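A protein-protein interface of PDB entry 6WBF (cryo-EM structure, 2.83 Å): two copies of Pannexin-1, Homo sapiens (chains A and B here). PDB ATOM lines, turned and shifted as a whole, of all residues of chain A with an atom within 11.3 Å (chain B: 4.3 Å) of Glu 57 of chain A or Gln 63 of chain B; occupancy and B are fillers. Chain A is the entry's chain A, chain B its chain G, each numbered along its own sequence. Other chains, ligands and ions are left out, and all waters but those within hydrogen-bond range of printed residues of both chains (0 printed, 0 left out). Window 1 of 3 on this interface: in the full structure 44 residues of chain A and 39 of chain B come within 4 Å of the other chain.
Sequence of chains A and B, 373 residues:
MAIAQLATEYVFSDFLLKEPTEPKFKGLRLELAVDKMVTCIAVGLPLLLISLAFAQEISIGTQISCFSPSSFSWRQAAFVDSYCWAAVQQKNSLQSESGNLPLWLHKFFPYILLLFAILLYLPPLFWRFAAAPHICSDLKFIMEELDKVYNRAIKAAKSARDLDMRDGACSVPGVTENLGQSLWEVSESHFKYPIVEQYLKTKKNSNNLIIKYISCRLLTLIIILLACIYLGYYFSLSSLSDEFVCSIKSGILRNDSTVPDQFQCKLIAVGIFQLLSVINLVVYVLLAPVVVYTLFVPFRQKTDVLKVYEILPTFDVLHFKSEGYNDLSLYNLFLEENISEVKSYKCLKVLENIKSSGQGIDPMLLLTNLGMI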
ATOM      1  N   ALA A   2      20.161  15.287  14.479  1.00  0.00           N
ATOM      2  CA  ALA A   2      18.928  14.776  15.058  1.00  0.00           C
ATOM      3  C   ALA A   2      18.210  13.863  14.078  1.00  0.00           C
ATOM      4  O   ALA A   2      18.292  14.052  12.869  1.00  0.00           O
ATOM      5  CB  ALA A   2      18.023  15.919  15.475  1.00  0.00           C
ATOM      6  N   ILE A   3      17.500  12.872  14.617  1.00  0.00           N
ATOM      7  CA  ILE A   3      16.751  11.938  13.781  1.00  0.00           C
ATOM      8  C   ILE A   3      15.724  12.670  12.931  1.00  0.00           C
ATOM      9  O   ILE A   3      15.591  12.408  11.729  1.00  0.00           O
ATOM     10  CB  ILE A   3      16.101  10.854  14.657  1.00  0.00           C
ATOM     11  CG1 ILE A   3      17.049   9.670  14.830  1.00  0.00           C
ATOM     12  CG2 ILE A   3      14.788  10.400  14.084  1.00  0.00           C
ATOM     13  CD1 ILE A   3      17.263   8.897  13.577  1.00  0.00           C
ATOM     14  N   ALA A   4      14.979  13.594  13.534  1.00  0.00           N
ATOM     15  CA  ALA A   4      13.905  14.251  12.802  1.00  0.00           C
ATOM     16  C   ALA A   4      14.449  15.141  11.695  1.00  0.00           C
ATOM     17  O   ALA A   4      13.812  15.301  10.649  1.00  0.00           O
ATOM     18  CB  ALA A   4      13.035  15.047  13.768  1.00  0.00           C
ATOM     19  N   GLN A   5      15.639  15.714  11.894  1.00  0.00           N
ATOM     20  CA  GLN A   5      16.249  16.510  10.834  1.00  0.00           C
ATOM     21  C   GLN A   5      16.571  15.649   9.621  1.00  0.00           C
ATOM     22  O   GLN A   5      16.290  16.038   8.481  1.00  0.00           O
ATOM     23  CB  GLN A   5      17.510  17.198  11.348  1.00  0.00           C
ATOM     24  CG  GLN A   5      17.253  18.243  12.409  1.00  0.00           C
ATOM     25  CD  GLN A   5      18.507  19.002  12.784  1.00  0.00           C
ATOM     26  OE1 GLN A   5      19.437  19.119  11.986  1.00  0.00           O
ATOM     27  NE2 GLN A   5      18.541  19.520  14.005  1.00  0.00           N
ATOM     28  N   LEU A   6      17.163  14.476   9.849  1.00  0.00           N
ATOM     29  CA  LEU A   6      17.441  13.561   8.749  1.00  0.00           C
ATOM     30  C   LEU A   6      16.155  13.096   8.088  1.00  0.00           C
ATOM     31  O   LEU A   6      16.087  12.971   6.859  1.00  0.00           O
ATOM     32  CB  LEU A   6      18.241  12.366   9.254  1.00  0.00           C
ATOM     33  CG  LEU A   6      19.419  12.731  10.150  1.00  0.00           C
ATOM     34  CD1 LEU A   6      19.958  11.500  10.851  1.00  0.00           C
ATOM     35  CD2 LEU A   6      20.505  13.412   9.339  1.00  0.00           C
ATOM     36  N   ALA A   7      15.124  12.831   8.890  1.00  0.00           N
ATOM     37  CA  ALA A   7      13.834  12.453   8.333  1.00  0.00           C
ATOM     38  C   ALA A   7      13.325  13.520   7.378  1.00  0.00           C
ATOM     39  O   ALA A   7      12.988  13.230   6.228  1.00  0.00           O
ATOM     40  CB  ALA A   7      12.827  12.203   9.453  1.00  0.00           C
ATOM     41  N   LEU A  48      19.954   7.883   4.075  1.00  0.00           N
ATOM     42  CA  LEU A  48      19.161   8.051   5.319  1.00  0.00           C
ATOM     43  C   LEU A  48      19.627   7.024   6.354  1.00  0.00           C
ATOM     44  O   LEU A  48      19.663   7.372   7.538  1.00  0.00           O
ATOM     45  CB  LEU A  48      17.671   7.878   5.015  1.00  0.00           C
ATOM     46  CG  LEU A  48      16.779   7.727   6.244  1.00  0.00           C
ATOM     47  CD1 LEU A  48      16.368   9.082   6.791  1.00  0.00           C
ATOM     48  CD2 LEU A  48      15.559   6.877   5.937  1.00  0.00           C
ATOM     49  N   ILE A  50      22.695   5.580   6.517  1.00  0.00           N
ATOM     50  CA  ILE A  50      23.993   6.026   7.014  1.00  0.00           C
ATOM     51  C   ILE A  50      23.807   7.086   8.085  1.00  0.00           C
ATOM     52  O   ILE A  50      24.416   7.020   9.159  1.00  0.00           O
ATOM     53  CB  ILE A  50      24.861   6.554   5.861  1.00  0.00           C
ATOM     54  CG1 ILE A  50      25.346   5.416   4.979  1.00  0.00           C
ATOM     55  CG2 ILE A  50      26.044   7.315   6.405  1.00  0.00           C
ATOM     56  CD1 ILE A  50      25.965   5.907   3.701  1.00  0.00           C
ATOM     57  N   SER A  51      22.963   8.080   7.814  1.00  0.00           N
ATOM     58  CA  SER A  51      22.767   9.157   8.776  1.00  0.00           C
ATOM     59  C   SER A  51      22.126   8.657  10.061  1.00  0.00           C
ATOM     60  O   SER A  51      22.401   9.193  11.139  1.00  0.00           O
ATOM     61  CB  SER A  51      21.921  10.257   8.150  1.00  0.00           C
ATOM     62  OG  SER A  51      22.555  10.780   7.001  1.00  0.00           O
ATOM     63  N   LEU A  52      21.276   7.638   9.972  1.00  0.00           N
ATOM     64  CA  LEU A  52      20.676   7.060  11.170  1.00  0.00           C
ATOM     65  C   LEU A  52      21.687   6.248  11.964  1.00  0.00           C
ATOM     66  O   LEU A  52      21.683   6.289  13.199  1.00  0.00           O
ATOM     67  CB  LEU A  52      19.477   6.196  10.791  1.00  0.00           C
ATOM     68  CG  LEU A  52      18.084   6.820  10.812  1.00  0.00           C
ATOM     69  CD1 LEU A  52      17.930   7.955   9.836  1.00  0.00           C
ATOM     70  CD2 LEU A  52      17.073   5.747  10.499  1.00  0.00           C
ATOM     71  N   ALA A  53      22.560   5.507  11.280  1.00  0.00           N
ATOM     72  CA  ALA A  53      23.481   4.617  11.978  1.00  0.00           C
ATOM     73  C   ALA A  53      24.395   5.377  12.925  1.00  0.00           C
ATOM     74  O   ALA A  53      25.025   4.771  13.797  1.00  0.00           O
ATOM     75  CB  ALA A  53      24.308   3.823  10.971  1.00  0.00           C
ATOM     76  N   PHE A  54      24.484   6.696  12.773  1.00  0.00           N
ATOM     77  CA  PHE A  54      25.300   7.525  13.645  1.00  0.00           C
ATOM     78  C   PHE A  54      24.520   8.695  14.221  1.00  0.00           C
ATOM     79  O   PHE A  54      25.117   9.712  14.586  1.00  0.00           O
ATOM     80  CB  PHE A  54      26.531   8.012  12.892  1.00  0.00           C
ATOM     81  CG  PHE A  54      27.318   6.905  12.285  1.00  0.00           C
ATOM     82  CD1 PHE A  54      28.108   6.095  13.075  1.00  0.00           C
ATOM     83  CD2 PHE A  54      27.240   6.646  10.937  1.00  0.00           C
ATOM     84  CE1 PHE A  54      28.819   5.062  12.526  1.00  0.00           C
ATOM     85  CE2 PHE A  54      27.949   5.619  10.385  1.00  0.00           C
ATOM     86  CZ  PHE A  54      28.742   4.826  11.179  1.00  0.00           C
ATOM     87  N   ALA A  55      23.198   8.577  14.289  1.00  0.00           N
ATOM     88  CA  ALA A  55      22.406   9.551  15.019  1.00  0.00           C
ATOM     89  C   ALA A  55      22.945   9.679  16.435  1.00  0.00           C
ATOM     90  O   ALA A  55      23.313   8.688  17.067  1.00  0.00           O
ATOM     91  CB  ALA A  55      20.938   9.136  15.044  1.00  0.00           C
ATOM     92  N   GLN A  56      22.998  10.915  16.931  1.00  0.00           N
ATOM     93  CA  GLN A  56      23.702  11.174  18.180  1.00  0.00           C
ATOM     94  C   GLN A  56      23.089  10.417  19.351  1.00  0.00           C
ATOM     95  O   GLN A  56      23.743  10.236  20.383  1.00  0.00           O
ATOM     96  CB  GLN A  56      23.719  12.675  18.468  1.00  0.00           C
ATOM     97  CG  GLN A  56      24.717  13.080  19.535  1.00  0.00           C
ATOM     98  CD  GLN A  56      26.096  12.516  19.271  1.00  0.00           C
ATOM     99  OE1 GLN A  56      26.512  11.544  19.899  1.00  0.00           O
ATOM    100  NE2 GLN A  56      26.814  13.122  18.332  1.00  0.00           N
ATOM    101  N   GLU A  57      21.844   9.961  19.213  1.00  0.00           N
ATOM    102  CA  GLU A  57      21.202   9.263  20.321  1.00  0.00           C
ATOM    103  C   GLU A  57      21.305   7.752  20.175  1.00  0.00           C
ATOM    104  O   GLU A  57      21.041   7.010  21.125  1.00  0.00           O
ATOM    105  CB  GLU A  57      19.749   9.691  20.442  1.00  0.00           C
ATOM    106  CG  GLU A  57      18.879   9.331  19.279  1.00  0.00           C
ATOM    107  CD  GLU A  57      18.819  10.443  18.266  1.00  0.00           C
ATOM    108  OE1 GLU A  57      19.736  11.287  18.247  1.00  0.00           O
ATOM    109  OE2 GLU A  57      17.824  10.506  17.525  1.00  0.00           O
ATOM    110  N   ILE A  58      21.659   7.271  18.988  1.00  0.00           N
ATOM    111  CA  ILE A  58      21.878   5.836  18.836  1.00  0.00           C
ATOM    112  C   ILE A  58      23.349   5.505  19.041  1.00  0.00           C
ATOM    113  O   ILE A  58      23.695   4.417  19.512  1.00  0.00           O
ATOM    114  CB  ILE A  58      21.355   5.368  17.470  1.00  0.00           C
ATOM    115  CG1 ILE A  58      19.844   5.540  17.419  1.00  0.00           C
ATOM    116  CG2 ILE A  58      21.666   3.917  17.250  1.00  0.00           C
ATOM    117  CD1 ILE A  58      19.110   4.625  18.367  1.00  0.00           C
ATOM    118  N   SER A  59      24.232   6.445  18.725  1.00  0.00           N
ATOM    119  CA  SER A  59      25.660   6.271  18.962  1.00  0.00           C
ATOM    120  C   SER A  59      25.948   6.496  20.439  1.00  0.00           C
ATOM    121  O   SER A  59      25.581   7.531  21.001  1.00  0.00           O
ATOM    122  CB  SER A  59      26.465   7.233  18.095  1.00  0.00           C
ATOM    123  OG  SER A  59      26.284   6.945  16.722  1.00  0.00           O
ATOM    124  N   ILE A  60      26.606   5.527  21.074  1.00  0.00           N
ATOM    125  CA  ILE A  60      26.995   5.694  22.470  1.00  0.00           C
ATOM    126  C   ILE A  60      28.264   6.526  22.571  1.00  0.00           C
ATOM    127  O   ILE A  60      28.507   7.196  23.581  1.00  0.00           O
ATOM    128  CB  ILE A  60      27.160   4.323  23.148  1.00  0.00           C
ATOM    129  CG1 ILE A  60      27.348   4.492  24.651  1.00  0.00           C
ATOM    130  CG2 ILE A  60      28.337   3.575  22.556  1.00  0.00           C
ATOM    131  CD1 ILE A  60      26.308   5.369  25.289  1.00  0.00           C
ATOM    132  N   GLY A  61      29.085   6.512  21.529  1.00  0.00           N
ATOM    133  CA  GLY A  61      30.365   7.183  21.573  1.00  0.00           C
ATOM    134  C   GLY A  61      31.256   6.757  20.430  1.00  0.00           C
ATOM    135  O   GLY A  61      30.861   6.833  19.263  1.00  0.00           O
ATOM    136  N   THR A  62      32.466   6.312  20.754  1.00  0.00           N
ATOM    137  CA  THR A  62      33.382   5.839  19.729  1.00  0.00           C
ATOM    138  C   THR A  62      32.811   4.621  19.018  1.00  0.00           C
ATOM    139  O   THR A  62      31.865   3.984  19.487  1.00  0.00           O
ATOM    140  CB  THR A  62      34.738   5.495  20.340  1.00  0.00           C
ATOM    141  OG1 THR A  62      34.568   4.470  21.324  1.00  0.00           O
ATOM    142  CG2 THR A  62      35.354   6.721  20.988  1.00  0.00           C
ATOM    143  N   ILE A 268      31.529  -1.269  18.294  1.00  0.00           N
ATOM    144  CA  ILE A 268      30.195  -0.782  18.600  1.00  0.00           C
ATOM    145  C   ILE A 268      29.509  -0.375  17.304  1.00  0.00           C
ATOM    146  O   ILE A 268      30.156  -0.153  16.272  1.00  0.00           O
ATOM    147  CB  ILE A 268      30.258   0.394  19.590  1.00  0.00           C
ATOM    148  CG1 ILE A 268      31.354   0.165  20.624  1.00  0.00           C
ATOM    149  CG2 ILE A 268      28.938   0.563  20.300  1.00  0.00           C
ATOM    150  CD1 ILE A 268      31.141  -1.061  21.471  1.00  0.00           C
ATOM    151  N   ALA A 269      28.182  -0.295  17.347  1.00  0.00           N
ATOM    152  CA  ALA A 269      27.345   0.104  16.226  1.00  0.00           C
ATOM    153  C   ALA A 269      27.403  -0.875  15.067  1.00  0.00           C
ATOM    154  O   ALA A 269      27.091  -0.497  13.938  1.00  0.00           O
ATOM    155  CB  ALA A 269      27.691   1.508  15.719  1.00  0.00           C
ATOM    156  N   ILE A 272      23.682  -2.080  14.979  1.00  0.00           N
ATOM    157  CA  ILE A 272      22.927  -1.068  14.252  1.00  0.00           C
ATOM    158  C   ILE A 272      23.159  -1.209  12.757  1.00  0.00           C
ATOM    159  O   ILE A 272      22.229  -1.075  11.955  1.00  0.00           O
ATOM    160  CB  ILE A 272      23.310   0.334  14.752  1.00  0.00           C
ATOM    161  CG1 ILE A 272      23.131   0.407  16.264  1.00  0.00           C
ATOM    162  CG2 ILE A 272      22.473   1.385  14.068  1.00  0.00           C
ATOM    163  CD1 ILE A 272      24.049   1.387  16.932  1.00  0.00           C
ATOM    164  N   PHE B  54      15.254  13.618  23.171  1.00  0.00           N
ATOM    165  CA  PHE B  54      16.677  13.884  23.291  1.00  0.00           C
ATOM    166  C   PHE B  54      16.983  15.373  23.339  1.00  0.00           C
ATOM    167  O   PHE B  54      18.091  15.784  22.989  1.00  0.00           O
ATOM    168  CB  PHE B  54      17.430  13.212  22.150  1.00  0.00           C
ATOM    169  CG  PHE B  54      17.146  11.755  22.045  1.00  0.00           C
ATOM    170  CD1 PHE B  54      17.698  10.870  22.946  1.00  0.00           C
ATOM    171  CD2 PHE B  54      16.298  11.275  21.076  1.00  0.00           C
ATOM    172  CE1 PHE B  54      17.428   9.531  22.867  1.00  0.00           C
ATOM    173  CE2 PHE B  54      16.025   9.939  20.991  1.00  0.00           C
ATOM    174  CZ  PHE B  54      16.593   9.065  21.887  1.00  0.00           C
ATOM    175  N   GLY B  61      22.767  12.719  29.542  1.00  0.00           N
ATOM    176  CA  GLY B  61      24.039  12.351  28.957  1.00  0.00           C
ATOM    177  C   GLY B  61      23.903  11.162  28.035  1.00  0.00           C
ATOM    178  O   GLY B  61      23.084  11.174  27.113  1.00  0.00           O
ATOM    179  N   THR B  62      24.708  10.133  28.271  1.00  0.00           N
ATOM    180  CA  THR B  62      24.626   8.926  27.464  1.00  0.00           C
ATOM    181  C   THR B  62      23.263   8.265  27.624  1.00  0.00           C
ATOM    182  O   THR B  62      22.502   8.568  28.545  1.00  0.00           O
ATOM    183  CB  THR B  62      25.726   7.944  27.855  1.00  0.00           C
ATOM    184  OG1 THR B  62      25.583   7.595  29.236  1.00  0.00           O
ATOM    185  CG2 THR B  62      27.095   8.562  27.631  1.00  0.00           C
ATOM    186  N   GLN B  63      22.960   7.349  26.704  1.00  0.00           N
ATOM    187  CA  GLN B  63      21.679   6.659  26.747  1.00  0.00           C
ATOM    188  C   GLN B  63      21.738   5.434  27.641  1.00  0.00           C
ATOM    189  O   GLN B  63      20.695   4.861  27.974  1.00  0.00           O
ATOM    190  CB  GLN B  63      21.250   6.263  25.338  1.00  0.00           C
ATOM    191  CG  GLN B  63      21.323   7.399  24.344  1.00  0.00           C
ATOM    192  CD  GLN B  63      22.685   7.504  23.697  1.00  0.00           C
ATOM    193  OE1 GLN B  63      23.497   6.587  23.790  1.00  0.00           O
ATOM    194  NE2 GLN B  63      22.949   8.632  23.056  1.00  0.00           N
ATOM    195  N   ILE B  64      22.935   5.008  28.030  1.00  0.00           N
ATOM    196  CA  ILE B  64      23.118   3.831  28.866  1.00  0.00           C
ATOM    197  C   ILE B  64      24.218   4.127  29.876  1.00  0.00           C
ATOM    198  O   ILE B  64      25.155   4.874  29.581  1.00  0.00           O
ATOM    199  CB  ILE B  64      23.461   2.590  28.026  1.00  0.00           C
ATOM    200  CG1 ILE B  64      23.519   1.342  28.896  1.00  0.00           C
ATOM    201  CG2 ILE B  64      24.774   2.778  27.308  1.00  0.00           C
ATOM    202  CD1 ILE B  64      23.804   0.092  28.122  1.00  0.00           C
ATOM    203  N   TRP B  85      25.754  -1.484  25.556  1.00  0.00           N
ATOM    204  CA  TRP B  85      24.929  -0.817  24.556  1.00  0.00           C
ATOM    205  C   TRP B  85      24.859  -1.631  23.275  1.00  0.00           C
ATOM    206  O   TRP B  85      23.782  -1.828  22.709  1.00  0.00           O
ATOM    207  CB  TRP B  85      25.486   0.573  24.276  1.00  0.00           C
ATOM    208  CG  TRP B  85      24.706   1.350  23.282  1.00  0.00           C
ATOM    209  CD1 TRP B  85      25.114   1.731  22.045  1.00  0.00           C
ATOM    210  CD2 TRP B  85      23.380   1.857  23.442  1.00  0.00           C
ATOM    211  NE1 TRP B  85      24.126   2.443  21.420  1.00  0.00           N
ATOM    212  CE2 TRP B  85      23.049   2.533  22.259  1.00  0.00           C
ATOM    213  CE3 TRP B  85      22.441   1.803  24.468  1.00  0.00           C
ATOM    214  CZ2 TRP B  85      21.822   3.149  22.073  1.00  0.00           C
ATOM    215  CZ3 TRP B  85      21.224   2.413  24.283  1.00  0.00           C
ATOM    216  CH2 TRP B  85      20.925   3.077  23.096  1.00  0.00           C
ATOM    217  N   PRO B 110      13.661   5.521  18.930  1.00  0.00           N
ATOM    218  CA  PRO B 110      13.632   6.594  17.927  1.00  0.00           C
ATOM    219  C   PRO B 110      13.497   6.075  16.513  1.00  0.00           C
ATOM    220  O   PRO B 110      12.783   6.673  15.699  1.00  0.00           O
ATOM    221  CB  PRO B 110      14.975   7.305  18.138  1.00  0.00           C
ATOM    222  CG  PRO B 110      15.405   6.917  19.481  1.00  0.00           C
ATOM    223  CD  PRO B 110      14.911   5.543  19.702  1.00  0.00           C
ATOM    224  N   LYS B 266      21.659   0.326  33.051  1.00  0.00           N
ATOM    225  CA  LYS B 266      20.332   0.918  32.967  1.00  0.00           C
ATOM    226  C   LYS B 266      20.253   1.789  31.726  1.00  0.00           C
ATOM    227  O   LYS B 266      21.156   2.587  31.467  1.00  0.00           O
ATOM    228  CB  LYS B 266      20.001   1.758  34.197  1.00  0.00           C
ATOM    229  CG  LYS B 266      18.589   2.306  34.170  1.00  0.00           C
ATOM    230  CD  LYS B 266      18.246   3.027  35.446  1.00  0.00           C
ATOM    231  CE  LYS B 266      16.802   3.474  35.448  1.00  0.00           C
ATOM    232  NZ  LYS B 266      15.882   2.317  35.535  1.00  0.00           N
ATOM    233  N   LEU B 267      19.177   1.631  30.968  1.00  0.00           N
ATOM    234  CA  LEU B 267      18.962   2.442  29.776  1.00  0.00           C
ATOM    235  C   LEU B 267      18.286   3.734  30.202  1.00  0.00           C
ATOM    236  O   LEU B 267      17.077   3.770  30.431  1.00  0.00           O
ATOM    237  CB  LEU B 267      18.129   1.690  28.752  1.00  0.00           C
ATOM    238  CG  LEU B 267      18.844   0.533  28.071  1.00  0.00           C
ATOM    239  CD1 LEU B 267      17.862  -0.245  27.252  1.00  0.00           C
ATOM    240  CD2 LEU B 267      19.958   1.047  27.199  1.00  0.00           C
ATOM    241  N   ILE B 268      19.074   4.797  30.324  1.00  0.00           N
ATOM    242  CA  ILE B 268      18.513   6.105  30.615  1.00  0.00           C
ATOM    243  C   ILE B 268      17.584   6.508  29.478  1.00  0.00           C
ATOM    244  O   ILE B 268      17.650   5.963  28.368  1.00  0.00           O
ATOM    245  CB  ILE B 268      19.625   7.146  30.820  1.00  0.00           C
ATOM    246  CG1 ILE B 268      20.805   6.526  31.561  1.00  0.00           C
ATOM    247  CG2 ILE B 268      19.113   8.327  31.608  1.00  0.00           C
ATOM    248  CD1 ILE B 268      20.464   6.030  32.939  1.00  0.00           C
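4 positions are printed for both chains. Of the 9 pairs that touch across the chains among the printed residues, none has its exchanged pair printed and touching as well.
Of chain B, only Phe 54 (3.4 Å) and Gln 63 (3.1 Å) come within 4 Å of Glu 57 of chain A. Gln 63 of chain B touches just these residues of chain A: Gln 56 (3.2 Å), Glu 57 (3.1 Å), Ser 59 (3.5 Å) and Ile 60 (3.4 Å). Of chain A, only Glu 57 (3.4 Å) comes within 4 Å of Phe 54 of chain B. No residue of chain A comes within 4 Å of Gly 61 of chain B. Printed residues of chain A within 4 Å of Thr 62 of chain B: Ile 60 (3.7 Å). Of the printed residues of chain A, Ile 64 of chain B touches Ile 60 (3.6 Å). Pro 110 of chain B touches none of the printed residues of chain A. No residue of chain A comes within 4 Å of Leu 267 of chain B. Printed residues of chain B within 4 Å of Ser 59 of chain A: Gln 63. Of the printed residues of chain B, Gln 56 of chain A touches Gln 63. Of the printed residues of chain A, Trp 85 of chain B touches Ile 58 and Ile 60. Ala 55 of chain A touches none of the printed residues of chain B. Gln 5 of chain A touches none of the printed residues of chain B.
The backbone carbonyl oxygen (O) of Ala 55 of chain A is in hydrogen-bond range of the side-chain hydroxyl (OG) of Ser 59 of chain A (3.5 Å). The side-chain hydroxyl (OG1) of Thr 62 of chain B lies within hydrogen-bond range of the backbone carbonyl oxygen (O) of Ile 64 of chain B, at 2.8 Å. The backbone carbonyl oxygen (O) of Gln 63 of chain B sits at hydrogen-bond distance from the backbone NH (N) of Ile 268 of chain B, at 2.9 Å.
Hydrophobic or aromatic side chains of chain A within 4 Å of the printed part of chain B: Ile 60. Hydrophobic or aromatic side chains of chain B within 4 Å of the printed part of chain A: Phe 54, Ile 64 and Trp 85. Among the printed residues, no Asp or Glu carboxylate lies within 4 Å of a Lys or Arg side-chain nitrogen of the other chain.
Phe 54 of chain B touches Glu 57 of chain A. O of Ser 59 of chain A touches NE2 of Gln 63 of chain B (3.5 Å). CB of Thr 62 of chain B touches CD1 of Ile 60 of chain A, 3.7 Å away. CD1 of Ile 60 of chain A touches OE1 of Gln 63 of chain B (3.4 Å). CD1 of Ile 60 of chain A touches CG2 of Ile 64 of chain B (3.6 Å). Trp 85 of chain B touches Ile 60 of chain A (CD1 to CB, 3.5 Å).
O of Gln 56 of chain A lies within hydrogen-bond range of NE2 of Gln 63 of chain B, 3.2 Å away. NE2 of Gln 63 of chain B lies close to O of Glu 57 of chain A (3.2 Å). NE1 of Trp 85 of chain B is in hydrogen-bond range of O of Ile 58 of chain A, 2.8 Å away.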
